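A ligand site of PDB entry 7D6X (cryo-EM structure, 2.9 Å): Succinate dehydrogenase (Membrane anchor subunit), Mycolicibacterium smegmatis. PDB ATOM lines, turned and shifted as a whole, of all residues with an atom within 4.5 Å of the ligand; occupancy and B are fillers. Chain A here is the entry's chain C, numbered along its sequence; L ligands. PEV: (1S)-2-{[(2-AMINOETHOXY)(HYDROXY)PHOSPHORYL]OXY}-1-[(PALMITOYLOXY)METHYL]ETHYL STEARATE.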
ATOM      1  N   LEU A  42      -7.444 -16.191  -5.807  1.00  0.00           N
ATOM      2  CA  LEU A  42      -7.277 -17.636  -5.956  1.00  0.00           C
ATOM      3  C   LEU A  42      -6.428 -17.972  -7.175  1.00  0.00           C
ATOM      4  O   LEU A  42      -5.568 -18.854  -7.117  1.00  0.00           O
ATOM      5  CB  LEU A  42      -8.630 -18.316  -6.045  1.00  0.00           C
ATOM      6  CG  LEU A  42      -9.472 -18.339  -4.774  1.00  0.00           C
ATOM      7  CD1 LEU A  42     -10.758 -19.122  -5.010  1.00  0.00           C
ATOM      8  CD2 LEU A  42      -8.686 -18.927  -3.631  1.00  0.00           C
ATOM      9  N   PHE A  45      -2.719 -17.142  -6.494  1.00  0.00           N
ATOM     10  CA  PHE A  45      -2.094 -18.104  -5.611  1.00  0.00           C
ATOM     11  C   PHE A  45      -1.846 -19.429  -6.315  1.00  0.00           C
ATOM     12  O   PHE A  45      -0.776 -20.024  -6.178  1.00  0.00           O
ATOM     13  CB  PHE A  45      -2.916 -18.351  -4.353  1.00  0.00           C
ATOM     14  CG  PHE A  45      -2.440 -19.525  -3.560  1.00  0.00           C
ATOM     15  CD1 PHE A  45      -1.268 -19.448  -2.835  1.00  0.00           C
ATOM     16  CD2 PHE A  45      -3.129 -20.716  -3.582  1.00  0.00           C
ATOM     17  CE1 PHE A  45      -0.814 -20.537  -2.115  1.00  0.00           C
ATOM     18  CE2 PHE A  45      -2.678 -21.802  -2.871  1.00  0.00           C
ATOM     19  CZ  PHE A  45      -1.518 -21.708  -2.137  1.00  0.00           C
ATOM     20  N   VAL A  46      -2.844 -19.938  -7.043  1.00  0.00           N
ATOM     21  CA  VAL A  46      -2.687 -21.244  -7.680  1.00  0.00           C
ATOM     22  C   VAL A  46      -1.600 -21.199  -8.737  1.00  0.00           C
ATOM     23  O   VAL A  46      -0.790 -22.131  -8.850  1.00  0.00           O
ATOM     24  CB  VAL A  46      -4.035 -21.726  -8.250  1.00  0.00           C
ATOM     25  CG1 VAL A  46      -3.842 -23.026  -8.995  1.00  0.00           C
ATOM     26  CG2 VAL A  46      -5.032 -21.932  -7.135  1.00  0.00           C
ATOM     27  N   ARG A 111      -7.590 -27.461   1.672  1.00  0.00           N
ATOM     28  CA  ARG A 111      -8.105 -26.129   1.382  1.00  0.00           C
ATOM     29  C   ARG A 111      -9.239 -26.173   0.370  1.00  0.00           C
ATOM     30  O   ARG A 111     -10.049 -25.240   0.328  1.00  0.00           O
ATOM     31  CB  ARG A 111      -6.984 -25.235   0.888  1.00  0.00           C
ATOM     32  CG  ARG A 111      -6.102 -24.743   1.999  1.00  0.00           C
ATOM     33  CD  ARG A 111      -5.196 -23.625   1.553  1.00  0.00           C
ATOM     34  NE  ARG A 111      -4.275 -23.247   2.620  1.00  0.00           N
ATOM     35  CZ  ARG A 111      -4.443 -22.212   3.425  1.00  0.00           C
ATOM     36  NH1 ARG A 111      -5.510 -21.437   3.288  1.00  0.00           N
ATOM     37  NH2 ARG A 111      -3.558 -21.959   4.367  1.00  0.00           N
ATOM     38  N   LEU A 112      -9.314 -27.219  -0.444  1.00  0.00           N
ATOM     39  CA  LEU A 112     -10.398 -27.333  -1.409  1.00  0.00           C
ATOM     40  C   LEU A 112     -11.709 -27.673  -0.718  1.00  0.00           C
ATOM     41  O   LEU A 112     -12.741 -27.054  -1.000  1.00  0.00           O
ATOM     42  CB  LEU A 112     -10.039 -28.401  -2.437  1.00  0.00           C
ATOM     43  CG  LEU A 112     -10.847 -28.455  -3.726  1.00  0.00           C
ATOM     44  CD1 LEU A 112     -10.283 -27.464  -4.717  1.00  0.00           C
ATOM     45  CD2 LEU A 112     -10.799 -29.863  -4.280  1.00  0.00           C
ATOM     46  N   TYR A 117     -13.613 -21.820   1.855  1.00  0.00           N
ATOM     47  CA  TYR A 117     -13.245 -21.835   0.445  1.00  0.00           C
ATOM     48  C   TYR A 117     -14.391 -22.328  -0.422  1.00  0.00           C
ATOM     49  O   TYR A 117     -14.569 -21.847  -1.541  1.00  0.00           O
ATOM     50  CB  TYR A 117     -12.014 -22.703   0.221  1.00  0.00           C
ATOM     51  CG  TYR A 117     -10.731 -22.004   0.581  1.00  0.00           C
ATOM     52  CD1 TYR A 117     -10.217 -21.008  -0.215  1.00  0.00           C
ATOM     53  CD2 TYR A 117     -10.056 -22.331   1.733  1.00  0.00           C
ATOM     54  CE1 TYR A 117      -9.053 -20.368   0.114  1.00  0.00           C
ATOM     55  CE2 TYR A 117      -8.889 -21.695   2.072  1.00  0.00           C
ATOM     56  CZ  TYR A 117      -8.395 -20.718   1.251  1.00  0.00           C
ATOM     57  OH  TYR A 117      -7.228 -20.081   1.589  1.00  0.00           O
ATOM     58  N   TYR A 121     -15.654 -20.202  -3.706  1.00  0.00           N
ATOM     59  CA  TYR A 121     -15.693 -20.561  -5.115  1.00  0.00           C
ATOM     60  C   TYR A 121     -17.078 -20.976  -5.593  1.00  0.00           C
ATOM     61  O   TYR A 121     -17.340 -20.860  -6.780  1.00  0.00           O
ATOM     62  CB  TYR A 121     -14.660 -21.631  -5.467  1.00  0.00           C
ATOM     63  CG  TYR A 121     -14.745 -22.986  -4.799  1.00  0.00           C
ATOM     64  CD1 TYR A 121     -13.752 -23.399  -3.928  1.00  0.00           C
ATOM     65  CD2 TYR A 121     -15.766 -23.869  -5.084  1.00  0.00           C
ATOM     66  CE1 TYR A 121     -13.798 -24.630  -3.335  1.00  0.00           C
ATOM     67  CE2 TYR A 121     -15.833 -25.102  -4.486  1.00  0.00           C
ATOM     68  CZ  TYR A 121     -14.841 -25.478  -3.623  1.00  0.00           C
ATOM     69  OH  TYR A 121     -14.884 -26.713  -3.022  1.00  0.00           O
ATOM     70  N   TYR A 122     -17.986 -21.390  -4.717  1.00  0.00           N
ATOM     71  CA  TYR A 122     -19.374 -21.552  -5.143  1.00  0.00           C
ATOM     72  C   TYR A 122     -19.955 -20.223  -5.581  1.00  0.00           C
ATOM     73  O   TYR A 122     -20.717 -20.166  -6.554  1.00  0.00           O
ATOM     74  CB  TYR A 122     -20.223 -22.142  -4.029  1.00  0.00           C
ATOM     75  CG  TYR A 122     -19.995 -23.604  -3.737  1.00  0.00           C
ATOM     76  CD1 TYR A 122     -19.574 -24.471  -4.730  1.00  0.00           C
ATOM     77  CD2 TYR A 122     -20.214 -24.121  -2.481  1.00  0.00           C
ATOM     78  CE1 TYR A 122     -19.370 -25.789  -4.465  1.00  0.00           C
ATOM     79  CE2 TYR A 122     -20.015 -25.439  -2.204  1.00  0.00           C
ATOM     80  CZ  TYR A 122     -19.593 -26.273  -3.196  1.00  0.00           C
ATOM     81  OH  TYR A 122     -19.390 -27.603  -2.924  1.00  0.00           O
ATOM     82  N   VAL A 125     -16.844 -19.017  -8.905  1.00  0.00           N
ATOM     83  CA  VAL A 125     -16.676 -19.812 -10.107  1.00  0.00           C
ATOM     84  C   VAL A 125     -17.997 -20.392 -10.555  1.00  0.00           C
ATOM     85  O   VAL A 125     -18.421 -20.204 -11.701  1.00  0.00           O
ATOM     86  CB  VAL A 125     -15.648 -20.932  -9.878  1.00  0.00           C
ATOM     87  CG1 VAL A 125     -15.518 -21.779 -11.121  1.00  0.00           C
ATOM     88  CG2 VAL A 125     -14.316 -20.358  -9.479  1.00  0.00           C
ATOM     89  N   TRP A 126     -18.664 -21.127  -9.660  1.00  0.00           N
ATOM     90  CA  TRP A 126     -19.847 -21.879 -10.059  1.00  0.00           C
ATOM     91  C   TRP A 126     -21.067 -21.005 -10.290  1.00  0.00           C
ATOM     92  O   TRP A 126     -22.073 -21.506 -10.780  1.00  0.00           O
ATOM     93  CB  TRP A 126     -20.167 -22.938  -9.010  1.00  0.00           C
ATOM     94  CG  TRP A 126     -21.138 -23.974  -9.490  1.00  0.00           C
ATOM     95  CD1 TRP A 126     -22.238 -24.426  -8.825  1.00  0.00           C
ATOM     96  CD2 TRP A 126     -21.117 -24.671 -10.745  1.00  0.00           C
ATOM     97  NE1 TRP A 126     -22.898 -25.375  -9.575  1.00  0.00           N
ATOM     98  CE2 TRP A 126     -22.220 -25.540 -10.757  1.00  0.00           C
ATOM     99  CE3 TRP A 126     -20.262 -24.659 -11.846  1.00  0.00           C
ATOM    100  CZ2 TRP A 126     -22.501 -26.378 -11.831  1.00  0.00           C
ATOM    101  CZ3 TRP A 126     -20.538 -25.488 -12.918  1.00  0.00           C
ATOM    102  CH2 TRP A 126     -21.653 -26.336 -12.896  1.00  0.00           C
ATOM    103  N   LYS A 140     -31.236 -25.637 -13.186  1.00  0.00           N
ATOM    104  CA  LYS A 140     -31.423 -26.711 -12.216  1.00  0.00           C
ATOM    105  C   LYS A 140     -30.290 -26.701 -11.205  1.00  0.00           C
ATOM    106  O   LYS A 140     -29.167 -26.310 -11.501  1.00  0.00           O
ATOM    107  CB  LYS A 140     -31.492 -28.072 -12.918  1.00  0.00           C
ATOM    108  CG  LYS A 140     -30.234 -28.434 -13.669  1.00  0.00           C
ATOM    109  CD  LYS A 140     -30.388 -29.724 -14.441  1.00  0.00           C
ATOM    110  CE  LYS A 140     -29.120 -30.077 -15.202  1.00  0.00           C
ATOM    111  NZ  LYS A 140     -28.856 -29.104 -16.300  1.00  0.00           N
ATOM    112  N   TYR A 141     -30.615 -27.144  -9.991  1.00  0.00           N
ATOM    113  CA  TYR A 141     -29.686 -27.102  -8.864  1.00  0.00           C
ATOM    114  C   TYR A 141     -29.935 -28.298  -7.976  1.00  0.00           C
ATOM    115  O   TYR A 141     -31.090 -28.600  -7.649  1.00  0.00           O
ATOM    116  CB  TYR A 141     -29.848 -25.805  -8.073  1.00  0.00           C
ATOM    117  CG  TYR A 141     -29.075 -25.722  -6.785  1.00  0.00           C
ATOM    118  CD1 TYR A 141     -27.747 -25.332  -6.776  1.00  0.00           C
ATOM    119  CD2 TYR A 141     -29.686 -25.996  -5.578  1.00  0.00           C
ATOM    120  CE1 TYR A 141     -27.056 -25.238  -5.603  1.00  0.00           C
ATOM    121  CE2 TYR A 141     -28.984 -25.909  -4.400  1.00  0.00           C
ATOM    122  CZ  TYR A 141     -27.681 -25.523  -4.418  1.00  0.00           C
ATOM    123  OH  TYR A 141     -26.992 -25.441  -3.238  1.00  0.00           O
ATOM    124  N   THR A 142     -28.865 -28.995  -7.589  1.00  0.00           N
ATOM    125  CA  THR A 142     -28.958 -30.142  -6.708  1.00  0.00           C
ATOM    126  C   THR A 142     -28.128 -30.001  -5.448  1.00  0.00           C
ATOM    127  O   THR A 142     -28.154 -30.910  -4.607  1.00  0.00           O
ATOM    128  CB  THR A 142     -28.550 -31.417  -7.440  1.00  0.00           C
ATOM    129  OG1 THR A 142     -27.145 -31.375  -7.728  1.00  0.00           O
ATOM    130  CG2 THR A 142     -29.312 -31.549  -8.739  1.00  0.00           C
ATOM    131  N   GLY A 143     -27.386 -28.914  -5.291  1.00  0.00           N
ATOM    132  CA  GLY A 143     -26.601 -28.703  -4.091  1.00  0.00           C
ATOM    133  C   GLY A 143     -25.503 -29.737  -3.940  1.00  0.00           C
ATOM    134  O   GLY A 143     -25.001 -30.308  -4.912  1.00  0.00           O
ATOM    135  N   PHE A 147     -23.284 -36.826  -6.859  1.00  0.00           N
ATOM    136  CA  PHE A 147     -22.017 -37.522  -6.608  1.00  0.00           C
ATOM    137  C   PHE A 147     -20.849 -36.587  -6.380  1.00  0.00           C
ATOM    138  O   PHE A 147     -20.298 -36.583  -5.255  1.00  0.00           O
ATOM    139  CB  PHE A 147     -21.724 -38.508  -7.752  1.00  0.00           C
ATOM    140  CG  PHE A 147     -20.262 -38.831  -7.873  1.00  0.00           C
ATOM    141  CD1 PHE A 147     -19.601 -39.490  -6.841  1.00  0.00           C
ATOM    142  CD2 PHE A 147     -19.539 -38.463  -8.990  1.00  0.00           C
ATOM    143  CE1 PHE A 147     -18.259 -39.778  -6.947  1.00  0.00           C
ATOM    144  CE2 PHE A 147     -18.197 -38.751  -9.095  1.00  0.00           C
ATOM    145  CZ  PHE A 147     -17.551 -39.412  -8.071  1.00  0.00           C
ATOM    146  N   PRO A 148     -20.404 -35.782  -7.339  1.00  0.00           N
ATOM    147  CA  PRO A 148     -19.093 -35.123  -7.168  1.00  0.00           C
ATOM    148  C   PRO A 148     -19.038 -34.199  -5.973  1.00  0.00           C
ATOM    149  O   PRO A 148     -17.945 -33.970  -5.433  1.00  0.00           O
ATOM    150  CB  PRO A 148     -18.902 -34.370  -8.493  1.00  0.00           C
ATOM    151  CG  PRO A 148     -20.276 -34.080  -8.931  1.00  0.00           C
ATOM    152  CD  PRO A 148     -21.101 -35.262  -8.534  1.00  0.00           C
ATOM    153  N   LEU A 149     -20.168 -33.672  -5.530  1.00  0.00           N
ATOM    154  CA  LEU A 149     -20.205 -32.725  -4.431  1.00  0.00           C
ATOM    155  C   LEU A 149     -20.637 -33.342  -3.117  1.00  0.00           C
ATOM    156  O   LEU A 149     -20.580 -32.668  -2.082  1.00  0.00           O
ATOM    157  CB  LEU A 149     -21.110 -31.549  -4.775  1.00  0.00           C
ATOM    158  CG  LEU A 149     -20.412 -30.273  -5.255  1.00  0.00           C
ATOM    159  CD1 LEU A 149     -19.456 -30.577  -6.394  1.00  0.00           C
ATOM    160  CD2 LEU A 149     -21.426 -29.240  -5.687  1.00  0.00           C
ATOM    161  N   LEU A 151     -18.869 -35.554  -1.888  1.00  0.00           N
ATOM    162  CA  LEU A 151     -17.549 -35.870  -1.365  1.00  0.00           C
ATOM    163  C   LEU A 151     -16.941 -34.723  -0.571  1.00  0.00           C
ATOM    164  O   LEU A 151     -15.816 -34.875  -0.084  1.00  0.00           O
ATOM    165  CB  LEU A 151     -16.613 -36.243  -2.513  1.00  0.00           C
ATOM    166  CG  LEU A 151     -16.567 -37.691  -2.982  1.00  0.00           C
ATOM    167  CD1 LEU A 151     -17.841 -38.078  -3.682  1.00  0.00           C
ATOM    168  CD2 LEU A 151     -15.389 -37.881  -3.911  1.00  0.00           C
ATOM    169  N   PHE A 158      -9.190 -34.750   5.777  1.00  0.00           N
ATOM    170  CA  PHE A 158      -8.158 -33.811   5.382  1.00  0.00           C
ATOM    171  C   PHE A 158      -7.789 -32.883   6.519  1.00  0.00           C
ATOM    172  O   PHE A 158      -6.686 -32.356   6.525  1.00  0.00           O
ATOM    173  CB  PHE A 158      -8.633 -33.032   4.164  1.00  0.00           C
ATOM    174  CG  PHE A 158      -8.891 -33.889   2.976  1.00  0.00           C
ATOM    175  CD1 PHE A 158      -7.926 -34.753   2.521  1.00  0.00           C
ATOM    176  CD2 PHE A 158     -10.107 -33.864   2.347  1.00  0.00           C
ATOM    177  CE1 PHE A 158      -8.151 -35.561   1.442  1.00  0.00           C
ATOM    178  CE2 PHE A 158     -10.348 -34.673   1.260  1.00  0.00           C
ATOM    179  CZ  PHE A 158      -9.361 -35.515   0.807  1.00  0.00           C
ATOM    180  N   LEU A 248      -2.477 -18.007   3.084  1.00  0.00           N
ATOM    181  CA  LEU A 248      -2.066 -17.976   1.677  1.00  0.00           C
ATOM    182  C   LEU A 248      -0.964 -16.933   1.478  1.00  0.00           C
ATOM    183  O   LEU A 248       0.058 -17.210   0.829  1.00  0.00           O
ATOM    184  CB  LEU A 248      -3.256 -17.674   0.779  1.00  0.00           C
ATOM    185  CG  LEU A 248      -4.310 -18.767   0.635  1.00  0.00           C
ATOM    186  CD1 LEU A 248      -5.255 -18.432  -0.501  1.00  0.00           C
ATOM    187  CD2 LEU A 248      -3.656 -20.110   0.414  1.00  0.00           C
HETATM  188  C48 PEV L   1      -6.018 -22.010  -1.720  1.00  0.00           C
HETATM  189  C47 PEV L   1      -6.656 -23.273  -2.295  1.00  0.00           C
HETATM  190  C46 PEV L   1      -8.170 -23.154  -2.368  1.00  0.00           C
HETATM  191  C45 PEV L   1      -8.731 -23.850  -3.595  1.00  0.00           C
HETATM  192  C44 PEV L   1      -8.872 -22.866  -4.746  1.00  0.00           C
HETATM  193  C43 PEV L   1      -9.031 -23.582  -6.077  1.00  0.00           C
HETATM  194  C42 PEV L   1     -10.187 -22.988  -6.876  1.00  0.00           C
HETATM  195  C41 PEV L   1     -11.175 -24.082  -7.261  1.00  0.00           C
HETATM  196  C40 PEV L   1     -12.024 -23.658  -8.447  1.00  0.00           C
HETATM  197  C39 PEV L   1     -12.580 -24.871  -9.171  1.00  0.00           C
HETATM  198  C38 PEV L   1     -13.664 -25.501  -8.312  1.00  0.00           C
HETATM  199  C37 PEV L   1     -15.001 -24.839  -8.556  1.00  0.00           C
HETATM  200  C36 PEV L   1     -16.146 -25.766  -8.167  1.00  0.00           C
HETATM  201  C35 PEV L   1     -17.480 -25.039  -8.099  1.00  0.00           C
HETATM  202  C34 PEV L   1     -18.616 -26.015  -8.374  1.00  0.00           C
HETATM  203  C33 PEV L   1     -18.360 -26.790  -9.661  1.00  0.00           C
HETATM  204  C32 PEV L   1     -18.463 -28.287  -9.428  1.00  0.00           C
HETATM  205  C31 PEV L   1     -19.855 -28.795  -9.785  1.00  0.00           C
HETATM  206  O31 PEV L   1     -20.787 -28.112  -9.563  1.00  0.00           O
HETATM  207  O2  PEV L   1     -20.020 -30.060 -10.344  1.00  0.00           O
HETATM  208  C2  PEV L   1     -20.564 -30.042 -11.629  1.00  0.00           C
HETATM  209  C1  PEV L   1     -21.906 -30.758 -11.635  1.00  0.00           C
HETATM  210  O3P PEV L   1     -22.907 -29.885 -11.189  1.00  0.00           O
HETATM  211  P   PEV L   1     -23.614 -30.219  -9.754  1.00  0.00           P
HETATM  212  O1P PEV L   1     -22.992 -29.384  -8.671  1.00  0.00           O
HETATM  213  O2P PEV L   1     -23.413 -31.682  -9.443  1.00  0.00           O
HETATM  214  O4P PEV L   1     -25.224 -29.888  -9.842  1.00  0.00           O
HETATM  215  C4  PEV L   1     -25.678 -28.704  -9.263  1.00  0.00           C
HETATM  216  C5  PEV L   1     -26.482 -27.975 -10.336  1.00  0.00           C
HETATM  217  N6  PEV L   1     -26.873 -28.912 -11.382  1.00  0.00           N
HETATM  218  C3  PEV L   1     -19.612 -30.749 -12.597  1.00  0.00           C
HETATM  219  O3  PEV L   1     -19.562 -32.104 -12.279  1.00  0.00           O
HETATM  220  C11 PEV L   1     -19.938 -32.946 -13.326  1.00  0.00           C
HETATM  221  O11 PEV L   1     -21.039 -32.907 -13.763  1.00  0.00           O
HETATM  222  C12 PEV L   1     -18.934 -33.921 -13.934  1.00  0.00           C
HETATM  223  C13 PEV L   1     -18.207 -34.754 -12.887  1.00  0.00           C
HETATM  224  C14 PEV L   1     -17.669 -36.042 -13.497  1.00  0.00           C
HETATM  225  C15 PEV L   1     -16.146 -36.100 -13.458  1.00  0.00           C
HETATM  226  C16 PEV L   1     -15.629 -37.511 -13.221  1.00  0.00           C
HETATM  227  C17 PEV L   1     -14.436 -37.519 -12.268  1.00  0.00           C
HETATM  228  C18 PEV L   1     -14.559 -36.473 -11.163  1.00  0.00           C
HETATM  229  C19 PEV L   1     -14.580 -37.137  -9.800  1.00  0.00           C
HETATM  230  C20 PEV L   1     -13.597 -36.507  -8.822  1.00  0.00           C
HETATM  231  C21 PEV L   1     -13.258 -37.472  -7.689  1.00  0.00           C
HETATM  232  C22 PEV L   1     -12.876 -36.770  -6.396  1.00  0.00           C
HETATM  233  C23 PEV L   1     -11.379 -36.890  -6.074  1.00  0.00           C
HETATM  234  C24 PEV L   1     -11.125 -36.785  -4.580  1.00  0.00           C
HETATM  235  C25 PEV L   1     -10.292 -35.564  -4.212  1.00  0.00           C
HETATM  236  C26 PEV L   1     -10.781 -34.914  -2.914  1.00  0.00           C
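O of Lys 140 sits close to N6 of the ligand (3.5 Å).
The side-chain hydroxyl (OG1) of Thr 142 lies within hydrogen-bond range of an oxygen (O4P) of the ligand (3.2 Å).
The indole nitrogen (NE1) of Trp 126 sits close to an oxygen (O31) of the ligand, at 3.5 Å.
The side-chain hydroxyl (OH) of Tyr 121 lies within hydrogen-bond range of the backbone carbonyl oxygen (O) of Leu 112, 3.0 Å away.
NH1 of Arg 111 is in hydrogen-bond range of OH of Tyr 117 (2.8 Å).
The backbone carbonyl oxygen of Tyr 121 is in hydrogen-bond range of the backbone NH of Trp 126 (3.2 Å).
Phe 45 touches the ligand (CE2 to C48, 3.5 Å).
CD of Arg 111 touches C48 of the ligand (3.7 Å).
Tyr 117 touches the ligand.
Tyr 121 touches the ligand (CD2 to C36, 3.6 Å).
Tyr 122 touches the ligand (CE1 to C34, 3.99 Å).
CA of Tyr 141 touches C5 of the ligand, at 3.6 Å.
Pro 148 touches the ligand.
Leu 149 touches the ligand (CD2 to O1P, 3.4 Å).
Leu 151 touches the ligand (CD2 to C22, 3.7 Å).
Leu 248 touches the ligand.
13 residues have an atom within 4 Å of the ligand: Phe 45, Arg 111, Tyr 117, Tyr 121, Tyr 122, Trp 126, Lys 140, Tyr 141, Thr 142, Pro 148, Leu 149, Leu 151 and Leu 248.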
